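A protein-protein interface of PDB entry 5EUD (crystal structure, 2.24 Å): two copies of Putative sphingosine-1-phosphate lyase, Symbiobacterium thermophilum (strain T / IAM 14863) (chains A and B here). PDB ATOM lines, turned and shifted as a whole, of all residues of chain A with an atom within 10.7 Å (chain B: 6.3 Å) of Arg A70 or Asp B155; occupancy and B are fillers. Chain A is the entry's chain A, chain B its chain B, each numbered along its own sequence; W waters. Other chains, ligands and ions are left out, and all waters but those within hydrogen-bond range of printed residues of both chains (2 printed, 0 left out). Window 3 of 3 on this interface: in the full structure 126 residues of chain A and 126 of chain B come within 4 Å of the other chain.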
ATOM      1  N   PRO A  66       0.083 -27.883   3.268  1.00  0.00           N
ATOM      2  CA  PRO A  66      -1.054 -26.958   3.437  1.00  0.00           C
ATOM      3  C   PRO A  66      -0.800 -25.878   4.496  1.00  0.00           C
ATOM      4  O   PRO A  66      -0.167 -26.160   5.499  1.00  0.00           O
ATOM      5  CB  PRO A  66      -2.218 -27.882   3.837  1.00  0.00           C
ATOM      6  CG  PRO A  66      -1.597 -29.174   4.224  1.00  0.00           C
ATOM      7  CD  PRO A  66      -0.325 -29.291   3.464  1.00  0.00           C
ATOM      8  N   SER A  67      -1.229 -24.639   4.251  1.00  0.00           N
ATOM      9  CA  SER A  67      -1.044 -23.588   5.244  1.00  0.00           C
ATOM     10  C   SER A  67      -2.194 -23.624   6.264  1.00  0.00           C
ATOM     11  O   SER A  67      -3.230 -24.219   5.978  1.00  0.00           O
ATOM     12  CB  SER A  67      -0.912 -22.221   4.583  1.00  0.00           C
ATOM     13  OG  SER A  67      -2.178 -21.681   4.252  1.00  0.00           O
ATOM     14  N   HIS A  68      -2.001 -23.030   7.459  1.00  0.00           N
ATOM     15  CA  HIS A  68      -3.015 -23.013   8.515  1.00  0.00           C
ATOM     16  C   HIS A  68      -3.165 -21.615   9.103  1.00  0.00           C
ATOM     17  O   HIS A  68      -2.364 -21.204   9.933  1.00  0.00           O
ATOM     18  CB  HIS A  68      -2.672 -24.033   9.618  1.00  0.00           C
ATOM     19  CG  HIS A  68      -2.478 -25.433   9.116  1.00  0.00           C
ATOM     20  ND1 HIS A  68      -3.553 -26.259   8.856  1.00  0.00           N
ATOM     21  CD2 HIS A  68      -1.339 -26.103   8.849  1.00  0.00           C
ATOM     22  CE1 HIS A  68      -3.040 -27.404   8.451  1.00  0.00           C
ATOM     23  NE2 HIS A  68      -1.712 -27.358   8.422  1.00  0.00           N
ATOM     24  N   ALA A  69      -4.185 -20.880   8.670  1.00  0.00           N
ATOM     25  CA  ALA A  69      -4.416 -19.535   9.186  1.00  0.00           C
ATOM     26  C   ALA A  69      -5.497 -19.561  10.253  1.00  0.00           C
ATOM     27  O   ALA A  69      -5.674 -18.582  10.986  1.00  0.00           O
ATOM     28  CB  ALA A  69      -4.789 -18.595   8.053  1.00  0.00           C
ATOM     29  N   ARG A  70      -6.182 -20.719  10.371  1.00  0.00           N
ATOM     30  CA  ARG A  70      -7.298 -20.983  11.275  1.00  0.00           C
ATOM     31  C   ARG A  70      -7.184 -22.403  11.767  1.00  0.00           C
ATOM     32  O   ARG A  70      -6.659 -23.257  11.040  1.00  0.00           O
ATOM     33  CB  ARG A  70      -8.627 -20.911  10.496  1.00  0.00           C
ATOM     34  CG  ARG A  70      -9.083 -19.557  10.011  1.00  0.00           C
ATOM     35  CD  ARG A  70     -10.228 -19.763   9.045  1.00  0.00           C
ATOM     36  NE  ARG A  70     -11.349 -18.848   9.275  1.00  0.00           N
ATOM     37  CZ  ARG A  70     -11.491 -17.662   8.688  1.00  0.00           C
ATOM     38  NH1 ARG A  70     -10.559 -17.207   7.857  1.00  0.00           N
ATOM     39  NH2 ARG A  70     -12.554 -16.911   8.946  1.00  0.00           N
ATOM     40  N   LEU A  71      -7.716 -22.690  12.978  1.00  0.00           N
ATOM     41  CA  LEU A  71      -7.693 -24.073  13.482  1.00  0.00           C
ATOM     42  C   LEU A  71      -8.536 -24.961  12.554  1.00  0.00           C
ATOM     43  O   LEU A  71      -9.644 -24.555  12.216  1.00  0.00           O
ATOM     44  CB  LEU A  71      -8.332 -24.156  14.882  1.00  0.00           C
ATOM     45  CG  LEU A  71      -7.486 -23.740  16.093  1.00  0.00           C
ATOM     46  CD1 LEU A  71      -8.399 -23.371  17.298  1.00  0.00           C
ATOM     47  CD2 LEU A  71      -6.505 -24.847  16.484  1.00  0.00           C
ATOM     48  N   PRO A  72      -8.115 -26.188  12.187  1.00  0.00           N
ATOM     49  CA  PRO A  72      -9.051 -27.071  11.459  1.00  0.00           C
ATOM     50  C   PRO A  72     -10.287 -27.341  12.348  1.00  0.00           C
ATOM     51  O   PRO A  72     -10.198 -27.202  13.572  1.00  0.00           O
ATOM     52  CB  PRO A  72      -8.237 -28.365  11.267  1.00  0.00           C
ATOM     53  CG  PRO A  72      -7.209 -28.336  12.360  1.00  0.00           C
ATOM     54  CD  PRO A  72      -6.860 -26.893  12.537  1.00  0.00           C
ATOM     55  N   ARG A  73     -11.433 -27.687  11.758  1.00  0.00           N
ATOM     56  CA  ARG A  73     -12.630 -27.969  12.567  1.00  0.00           C
ATOM     57  C   ARG A  73     -12.400 -29.268  13.330  1.00  0.00           C
ATOM     58  O   ARG A  73     -12.556 -29.313  14.545  1.00  0.00           O
ATOM     59  CB  ARG A  73     -13.893 -28.065  11.692  1.00  0.00           C
ATOM     60  CG  ARG A  73     -14.888 -26.943  11.980  1.00  0.00           C
ATOM     61  CD  ARG A  73     -16.176 -27.090  11.188  1.00  0.00           C
ATOM     62  NE  ARG A  73     -17.103 -28.051  11.796  1.00  0.00           N
ATOM     63  CZ  ARG A  73     -17.275 -29.305  11.387  1.00  0.00           C
ATOM     64  NH1 ARG A  73     -16.582 -29.777  10.356  1.00  0.00           N
ATOM     65  NH2 ARG A  73     -18.143 -30.096  12.002  1.00  0.00           N
ATOM     66  N   ALA A  74     -11.990 -30.307  12.613  1.00  0.00           N
ATOM     67  CA  ALA A  74     -11.688 -31.585  13.218  1.00  0.00           C
ATOM     68  C   ALA A  74     -10.166 -31.650  13.404  1.00  0.00           C
ATOM     69  O   ALA A  74      -9.422 -31.183  12.547  1.00  0.00           O
ATOM     70  CB  ALA A  74     -12.151 -32.710  12.295  1.00  0.00           C
ATOM     71  N   GLY A  75      -9.720 -32.245  14.497  1.00  0.00           N
ATOM     72  CA  GLY A  75      -8.297 -32.453  14.733  1.00  0.00           C
ATOM     73  C   GLY A  75      -7.677 -33.292  13.635  1.00  0.00           C
ATOM     74  O   GLY A  75      -8.316 -34.216  13.133  1.00  0.00           O
ATOM     75  N   LEU A  76      -6.469 -32.928  13.201  1.00  0.00           N
ATOM     76  CA  LEU A  76      -5.739 -33.639  12.152  1.00  0.00           C
ATOM     77  C   LEU A  76      -5.039 -34.891  12.732  1.00  0.00           C
ATOM     78  O   LEU A  76      -4.635 -34.847  13.894  1.00  0.00           O
ATOM     79  CB  LEU A  76      -4.729 -32.678  11.480  1.00  0.00           C
ATOM     80  CG  LEU A  76      -5.357 -31.611  10.570  1.00  0.00           C
ATOM     81  CD1 LEU A  76      -4.436 -30.417  10.386  1.00  0.00           C
ATOM     82  CD2 LEU A  76      -5.737 -32.192   9.209  1.00  0.00           C
ATOM     83  N   VAL A 508       1.356 -15.792   6.709  1.00  0.00           N
ATOM     84  CA  VAL A 508       0.676 -17.075   6.481  1.00  0.00           C
ATOM     85  C   VAL A 508      -0.091 -16.959   5.161  1.00  0.00           C
ATOM     86  O   VAL A 508      -1.002 -16.129   5.052  1.00  0.00           O
ATOM     87  CB  VAL A 508      -0.244 -17.540   7.641  1.00  0.00           C
ATOM     88  CG1 VAL A 508      -0.916 -18.868   7.309  1.00  0.00           C
ATOM     89  CG2 VAL A 508       0.538 -17.665   8.926  1.00  0.00           C
ATOM     90  N   HIS A 509       0.314 -17.759   4.153  1.00  0.00           N
ATOM     91  CA  HIS A 509      -0.319 -17.774   2.825  1.00  0.00           C
ATOM     92  C   HIS A 509      -0.333 -19.176   2.237  1.00  0.00           C
ATOM     93  O   HIS A 509      -1.354 -19.851   2.312  1.00  0.00           O
ATOM     94  CB  HIS A 509       0.351 -16.781   1.852  1.00  0.00           C
ATOM     95  CG  HIS A 509       0.119 -15.341   2.197  1.00  0.00           C
ATOM     96  ND1 HIS A 509       1.142 -14.536   2.659  1.00  0.00           N
ATOM     97  CD2 HIS A 509      -1.025 -14.618   2.166  1.00  0.00           C
ATOM     98  CE1 HIS A 509       0.595 -13.353   2.883  1.00  0.00           C
ATOM     99  NE2 HIS A 509      -0.706 -13.352   2.601  1.00  0.00           N
ATOM    100  N   GLU B 143       1.863 -19.762  11.962  1.00  0.00           N
ATOM    101  CA  GLU B 143       0.567 -20.435  11.971  1.00  0.00           C
ATOM    102  C   GLU B 143      -0.054 -20.494  13.357  1.00  0.00           C
ATOM    103  O   GLU B 143      -1.264 -20.313  13.454  1.00  0.00           O
ATOM    104  CB  GLU B 143       0.671 -21.794  11.280  1.00  0.00           C
ATOM    105  CG  GLU B 143       1.033 -21.589   9.804  1.00  0.00           C
ATOM    106  CD  GLU B 143       1.074 -22.804   8.899  1.00  0.00           C
ATOM    107  OE1 GLU B 143       1.118 -23.945   9.413  1.00  0.00           O
ATOM    108  OE2 GLU B 143       1.086 -22.605   7.662  1.00  0.00           O
ATOM    109  N   ALA B 146      -1.431 -16.900  13.748  1.00  0.00           N
ATOM    110  CA  ALA B 146      -2.595 -16.765  12.866  1.00  0.00           C
ATOM    111  C   ALA B 146      -3.807 -17.501  13.438  1.00  0.00           C
ATOM    112  O   ALA B 146      -4.868 -16.893  13.589  1.00  0.00           O
ATOM    113  CB  ALA B 146      -2.275 -17.275  11.451  1.00  0.00           C
ATOM    114  N   MET B 147      -3.636 -18.777  13.812  1.00  0.00           N
ATOM    115  CA  MET B 147      -4.732 -19.583  14.383  1.00  0.00           C
ATOM    116  C   MET B 147      -5.261 -19.015  15.704  1.00  0.00           C
ATOM    117  O   MET B 147      -6.477 -18.971  15.892  1.00  0.00           O
ATOM    118  CB  MET B 147      -4.336 -21.052  14.512  1.00  0.00           C
ATOM    119  CG  MET B 147      -4.079 -21.728  13.167  1.00  0.00           C
ATOM    120  SD  MET B 147      -3.888 -23.520  13.293  1.00  0.00           S
ATOM    121  CE  MET B 147      -2.192 -23.641  14.045  1.00  0.00           C
ATOM    122  N   ALA B 149      -4.985 -15.753  16.772  1.00  0.00           N
ATOM    123  CA  ALA B 149      -5.613 -14.472  16.409  1.00  0.00           C
ATOM    124  C   ALA B 149      -7.033 -14.692  15.923  1.00  0.00           C
ATOM    125  O   ALA B 149      -7.938 -14.065  16.460  1.00  0.00           O
ATOM    126  CB  ALA B 149      -4.801 -13.757  15.343  1.00  0.00           C
ATOM    127  N   HIS B 150      -7.230 -15.653  14.995  1.00  0.00           N
ATOM    128  CA  HIS B 150      -8.550 -16.023  14.472  1.00  0.00           C
ATOM    129  C   HIS B 150      -9.505 -16.499  15.588  1.00  0.00           C
ATOM    130  O   HIS B 150     -10.684 -16.132  15.585  1.00  0.00           O
ATOM    131  CB  HIS B 150      -8.459 -17.093  13.360  1.00  0.00           C
ATOM    132  CG  HIS B 150      -9.812 -17.467  12.840  1.00  0.00           C
ATOM    133  ND1 HIS B 150     -10.491 -18.567  13.330  1.00  0.00           N
ATOM    134  CD2 HIS B 150     -10.621 -16.804  11.984  1.00  0.00           C
ATOM    135  CE1 HIS B 150     -11.671 -18.560  12.730  1.00  0.00           C
ATOM    136  NE2 HIS B 150     -11.792 -17.523  11.909  1.00  0.00           N
ATOM    137  N   LEU B 152      -9.427 -15.613  18.639  1.00  0.00           N
ATOM    138  CA  LEU B 152      -9.692 -14.496  19.558  1.00  0.00           C
ATOM    139  C   LEU B 152     -10.304 -13.267  18.889  1.00  0.00           C
ATOM    140  O   LEU B 152     -10.043 -12.144  19.297  1.00  0.00           O
ATOM    141  CB  LEU B 152      -8.408 -14.132  20.347  1.00  0.00           C
ATOM    142  CG  LEU B 152      -7.893 -15.222  21.282  1.00  0.00           C
ATOM    143  CD1 LEU B 152      -6.480 -14.914  21.776  1.00  0.00           C
ATOM    144  CD2 LEU B 152      -8.855 -15.443  22.444  1.00  0.00           C
ATOM    145  N   GLY B 153     -11.125 -13.503  17.874  1.00  0.00           N
ATOM    146  CA  GLY B 153     -11.880 -12.470  17.174  1.00  0.00           C
ATOM    147  C   GLY B 153     -11.100 -11.551  16.261  1.00  0.00           C
ATOM    148  O   GLY B 153     -11.578 -10.455  15.970  1.00  0.00           O
ATOM    149  N   GLY B 154      -9.928 -12.006  15.798  1.00  0.00           N
ATOM    150  CA  GLY B 154      -9.033 -11.249  14.924  1.00  0.00           C
ATOM    151  C   GLY B 154      -9.620 -10.743  13.618  1.00  0.00           C
ATOM    152  O   GLY B 154      -9.226  -9.672  13.137  1.00  0.00           O
ATOM    153  N   ASP B 155     -10.551 -11.533  13.023  1.00  0.00           N
ATOM    154  CA  ASP B 155     -11.270 -11.223  11.776  1.00  0.00           C
ATOM    155  C   ASP B 155     -12.048  -9.914  11.883  1.00  0.00           C
ATOM    156  O   ASP B 155     -12.112  -9.159  10.912  1.00  0.00           O
ATOM    157  CB  ASP B 155     -12.244 -12.356  11.414  1.00  0.00           C
ATOM    158  CG  ASP B 155     -11.599 -13.600  10.825  1.00  0.00           C
ATOM    159  OD1 ASP B 155     -10.351 -13.639  10.732  1.00  0.00           O
ATOM    160  OD2 ASP B 155     -12.342 -14.532  10.458  1.00  0.00           O
ATOM    161  N   ALA B 156     -12.593  -9.634  13.086  1.00  0.00           N
ATOM    162  CA  ALA B 156     -13.348  -8.426  13.413  1.00  0.00           C
ATOM    163  C   ALA B 156     -12.500  -7.156  13.303  1.00  0.00           C
ATOM    164  O   ALA B 156     -13.058  -6.064  13.269  1.00  0.00           O
ATOM    165  CB  ALA B 156     -13.949  -8.549  14.803  1.00  0.00           C
ATOM    166  N   ALA B 157     -11.172  -7.295  13.208  1.00  0.00           N
ATOM    167  CA  ALA B 157     -10.250  -6.169  13.048  1.00  0.00           C
ATOM    168  C   ALA B 157      -9.810  -5.959  11.585  1.00  0.00           C
ATOM    169  O   ALA B 157      -8.942  -5.124  11.320  1.00  0.00           O
ATOM    170  CB  ALA B 157      -9.047  -6.340  13.953  1.00  0.00           C
ATOM    171  N   GLY B 158     -10.437  -6.688  10.657  1.00  0.00           N
ATOM    172  CA  GLY B 158     -10.193  -6.568   9.223  1.00  0.00           C
ATOM    173  C   GLY B 158      -8.913  -7.177   8.676  1.00  0.00           C
ATOM    174  O   GLY B 158      -8.515  -6.860   7.554  1.00  0.00           O
ATOM    175  N   GLY B 159      -8.283  -8.054   9.449  1.00  0.00           N
ATOM    176  CA  GLY B 159      -7.051  -8.723   9.043  1.00  0.00           C
ATOM    177  C   GLY B 159      -5.767  -8.032   9.463  1.00  0.00           C
ATOM    178  O   GLY B 159      -4.699  -8.406   8.971  1.00  0.00           O
ATOM    179  N   VAL B 161      -4.735  -7.891  12.760  1.00  0.00           N
ATOM    180  CA  VAL B 161      -4.292  -8.572  13.974  1.00  0.00           C
ATOM    181  C   VAL B 161      -3.019  -9.398  13.663  1.00  0.00           C
ATOM    182  O   VAL B 161      -2.981 -10.163  12.696  1.00  0.00           O
ATOM    183  CB  VAL B 161      -5.416  -9.383  14.693  1.00  0.00           C
ATOM    184  CG1 VAL B 161      -4.866 -10.138  15.894  1.00  0.00           C
ATOM    185  CG2 VAL B 161      -6.548  -8.470  15.151  1.00  0.00           C
ATOM    186  N   PHE B 298     -10.622  -9.320  20.445  1.00  0.00           N
ATOM    187  CA  PHE B 298     -10.570  -8.359  19.348  1.00  0.00           C
ATOM    188  C   PHE B 298     -11.943  -8.026  18.742  1.00  0.00           C
ATOM    189  O   PHE B 298     -12.016  -7.092  17.949  1.00  0.00           O
ATOM    190  CB  PHE B 298      -9.558  -8.779  18.279  1.00  0.00           C
ATOM    191  CG  PHE B 298      -8.122  -8.739  18.769  1.00  0.00           C
ATOM    192  CD1 PHE B 298      -7.476  -7.524  18.983  1.00  0.00           C
ATOM    193  CD2 PHE B 298      -7.395  -9.909  18.934  1.00  0.00           C
ATOM    194  CE1 PHE B 298      -6.135  -7.486  19.373  1.00  0.00           C
ATOM    195  CE2 PHE B 298      -6.067  -9.871  19.360  1.00  0.00           C
ATOM    196  CZ  PHE B 298      -5.441  -8.660  19.565  1.00  0.00           C
ATOM    197  N   LEU B 368      -3.179 -28.353  15.960  1.00  0.00           N
ATOM    198  CA  LEU B 368      -3.574 -29.135  14.783  1.00  0.00           C
ATOM    199  C   LEU B 368      -4.206 -30.469  15.106  1.00  0.00           C
ATOM    200  O   LEU B 368      -5.118 -30.865  14.399  1.00  0.00           O
ATOM    201  CB  LEU B 368      -2.407 -29.334  13.794  1.00  0.00           C
ATOM    202  CG  LEU B 368      -1.870 -28.096  13.031  1.00  0.00           C
ATOM    203  CD1 LEU B 368      -1.012 -28.538  11.873  1.00  0.00           C
ATOM    204  CD2 LEU B 368      -3.003 -27.210  12.475  1.00  0.00           C
HETATM  205  O   HOH W   1      -8.423 -20.389  14.437  1.00  0.00           O
HETATM  206  O   HOH W   2      -5.966 -15.897  11.292  1.00  0.00           O
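The backbone NH (N) of His A68 lies within hydrogen-bond range of the side-chain carboxylate (OE2) of Glu B143 (3.1 Å). The backbone carbonyl oxygen of Ala A69 sits at hydrogen-bond distance from the backbone NH of Met B147, at 3.5 Å. NE2 of His B150 lies within hydrogen-bond range of NE of Arg A70, 3.0 Å away. The guanidinium group (NH2) of Arg A70 lies within salt-bridge range of the side-chain carboxylate (OD2) of Asp B155, at 2.8 Å. The backbone NH (N) of Leu A76 is in hydrogen-bond range of the backbone carbonyl oxygen (O) of Leu B368, 2.7 Å away. O of Ala B146 sits close to O of Ala A69 (3.2 Å). O of Arg A70 sits close to SD of Met B147 (3.6 Å).
OG of Ser A67 lies within hydrogen-bond range of O of His A509. The side-chain carboxylate of Asp B155 sits close to a ring nitrogen (NE2) of His B150.
Among the printed residues, pairs that only touch across the chains: Ser A67 with Glu B143 (3.4 Å), His A68 with Met B147 (3.7 Å), His A68 with Leu B368 (3.7 Å), Ala A69 with His B150 (3.95 Å), Leu A71 with Met B147 (3.8 Å), Pro A72 with Leu B368 (3.9 Å), Gly A75 with Leu B368 (3.6 Å), Val A508 with Glu B143 (3.9 Å) and Val A508 with Ala B146 (3.8 Å).
Printed residues of chain B within 4 Å of Ser A67: Glu B143. Of the printed residues of chain B, Arg A70 touches Met B147 (3.5 Å), His B150 (3.0 Å) and Asp B155 (2.8 Å). Arg A73 touches none of the printed residues of chain B. Of the printed residues of chain B, Val A508 touches Glu B143 and Ala B146. Of the printed residues of chain A, Glu B143 touches Ser A67, His A68 and Val A508. Met B147 touches just these residues of chain A: His A68 (3.7 Å), Ala A69 (3.5 Å), Arg A70 (3.5 Å) and Leu A71 (3.8 Å). Ala B149 touches none of the printed residues of chain A. His B150 touches just these residues of chain A: Ala A69 (3.95 Å) and Arg A70 (3.0 Å). No residue of chain A comes within 4 Å of Gly B153. Of chain A, only Arg A70 comes within 4 Å of Asp B155. No residue of chain A comes within 4 Å of Ala B156. No residue of chain A comes within 4 Å of Gly B158. The nearest residue of chain B that does not touch Arg A70 is Ala B146 (5.0 Å).
Of the 13 printed residues of chain A, 9 touch a printed residue of chain B. Hydrophobic or aromatic side chains of chain A within 4 Å of the printed part of chain B: His A68, Pro A72, Leu A76 and Val A508. Hydrophobic or aromatic side chains of chain B within 4 Å of the printed part of chain A: Ala B146, Met B147, His B150 and Leu B368. Among the printed residues, Asp or Glu carboxylates within 4 Å of a Lys or Arg side-chain nitrogen of the other chain: Arg A70 with Asp B155 (2.8 Å).
No position is printed for both chains. Of the 16 pairs that touch across the chains among the printed residues, none has its exchanged pair printed and touching as well.
Water W2 bridges the backbone carbonyl oxygen of Ala A69 (2.7 Å) and the backbone carbonyl oxygen of Ala B146 (2.7 Å). Water W1 lies within hydrogen-bond range of O of Met B147 (2.8 Å), N of Leu A71 (2.8 Å) and ND1 of His B150 (3.0 Å).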
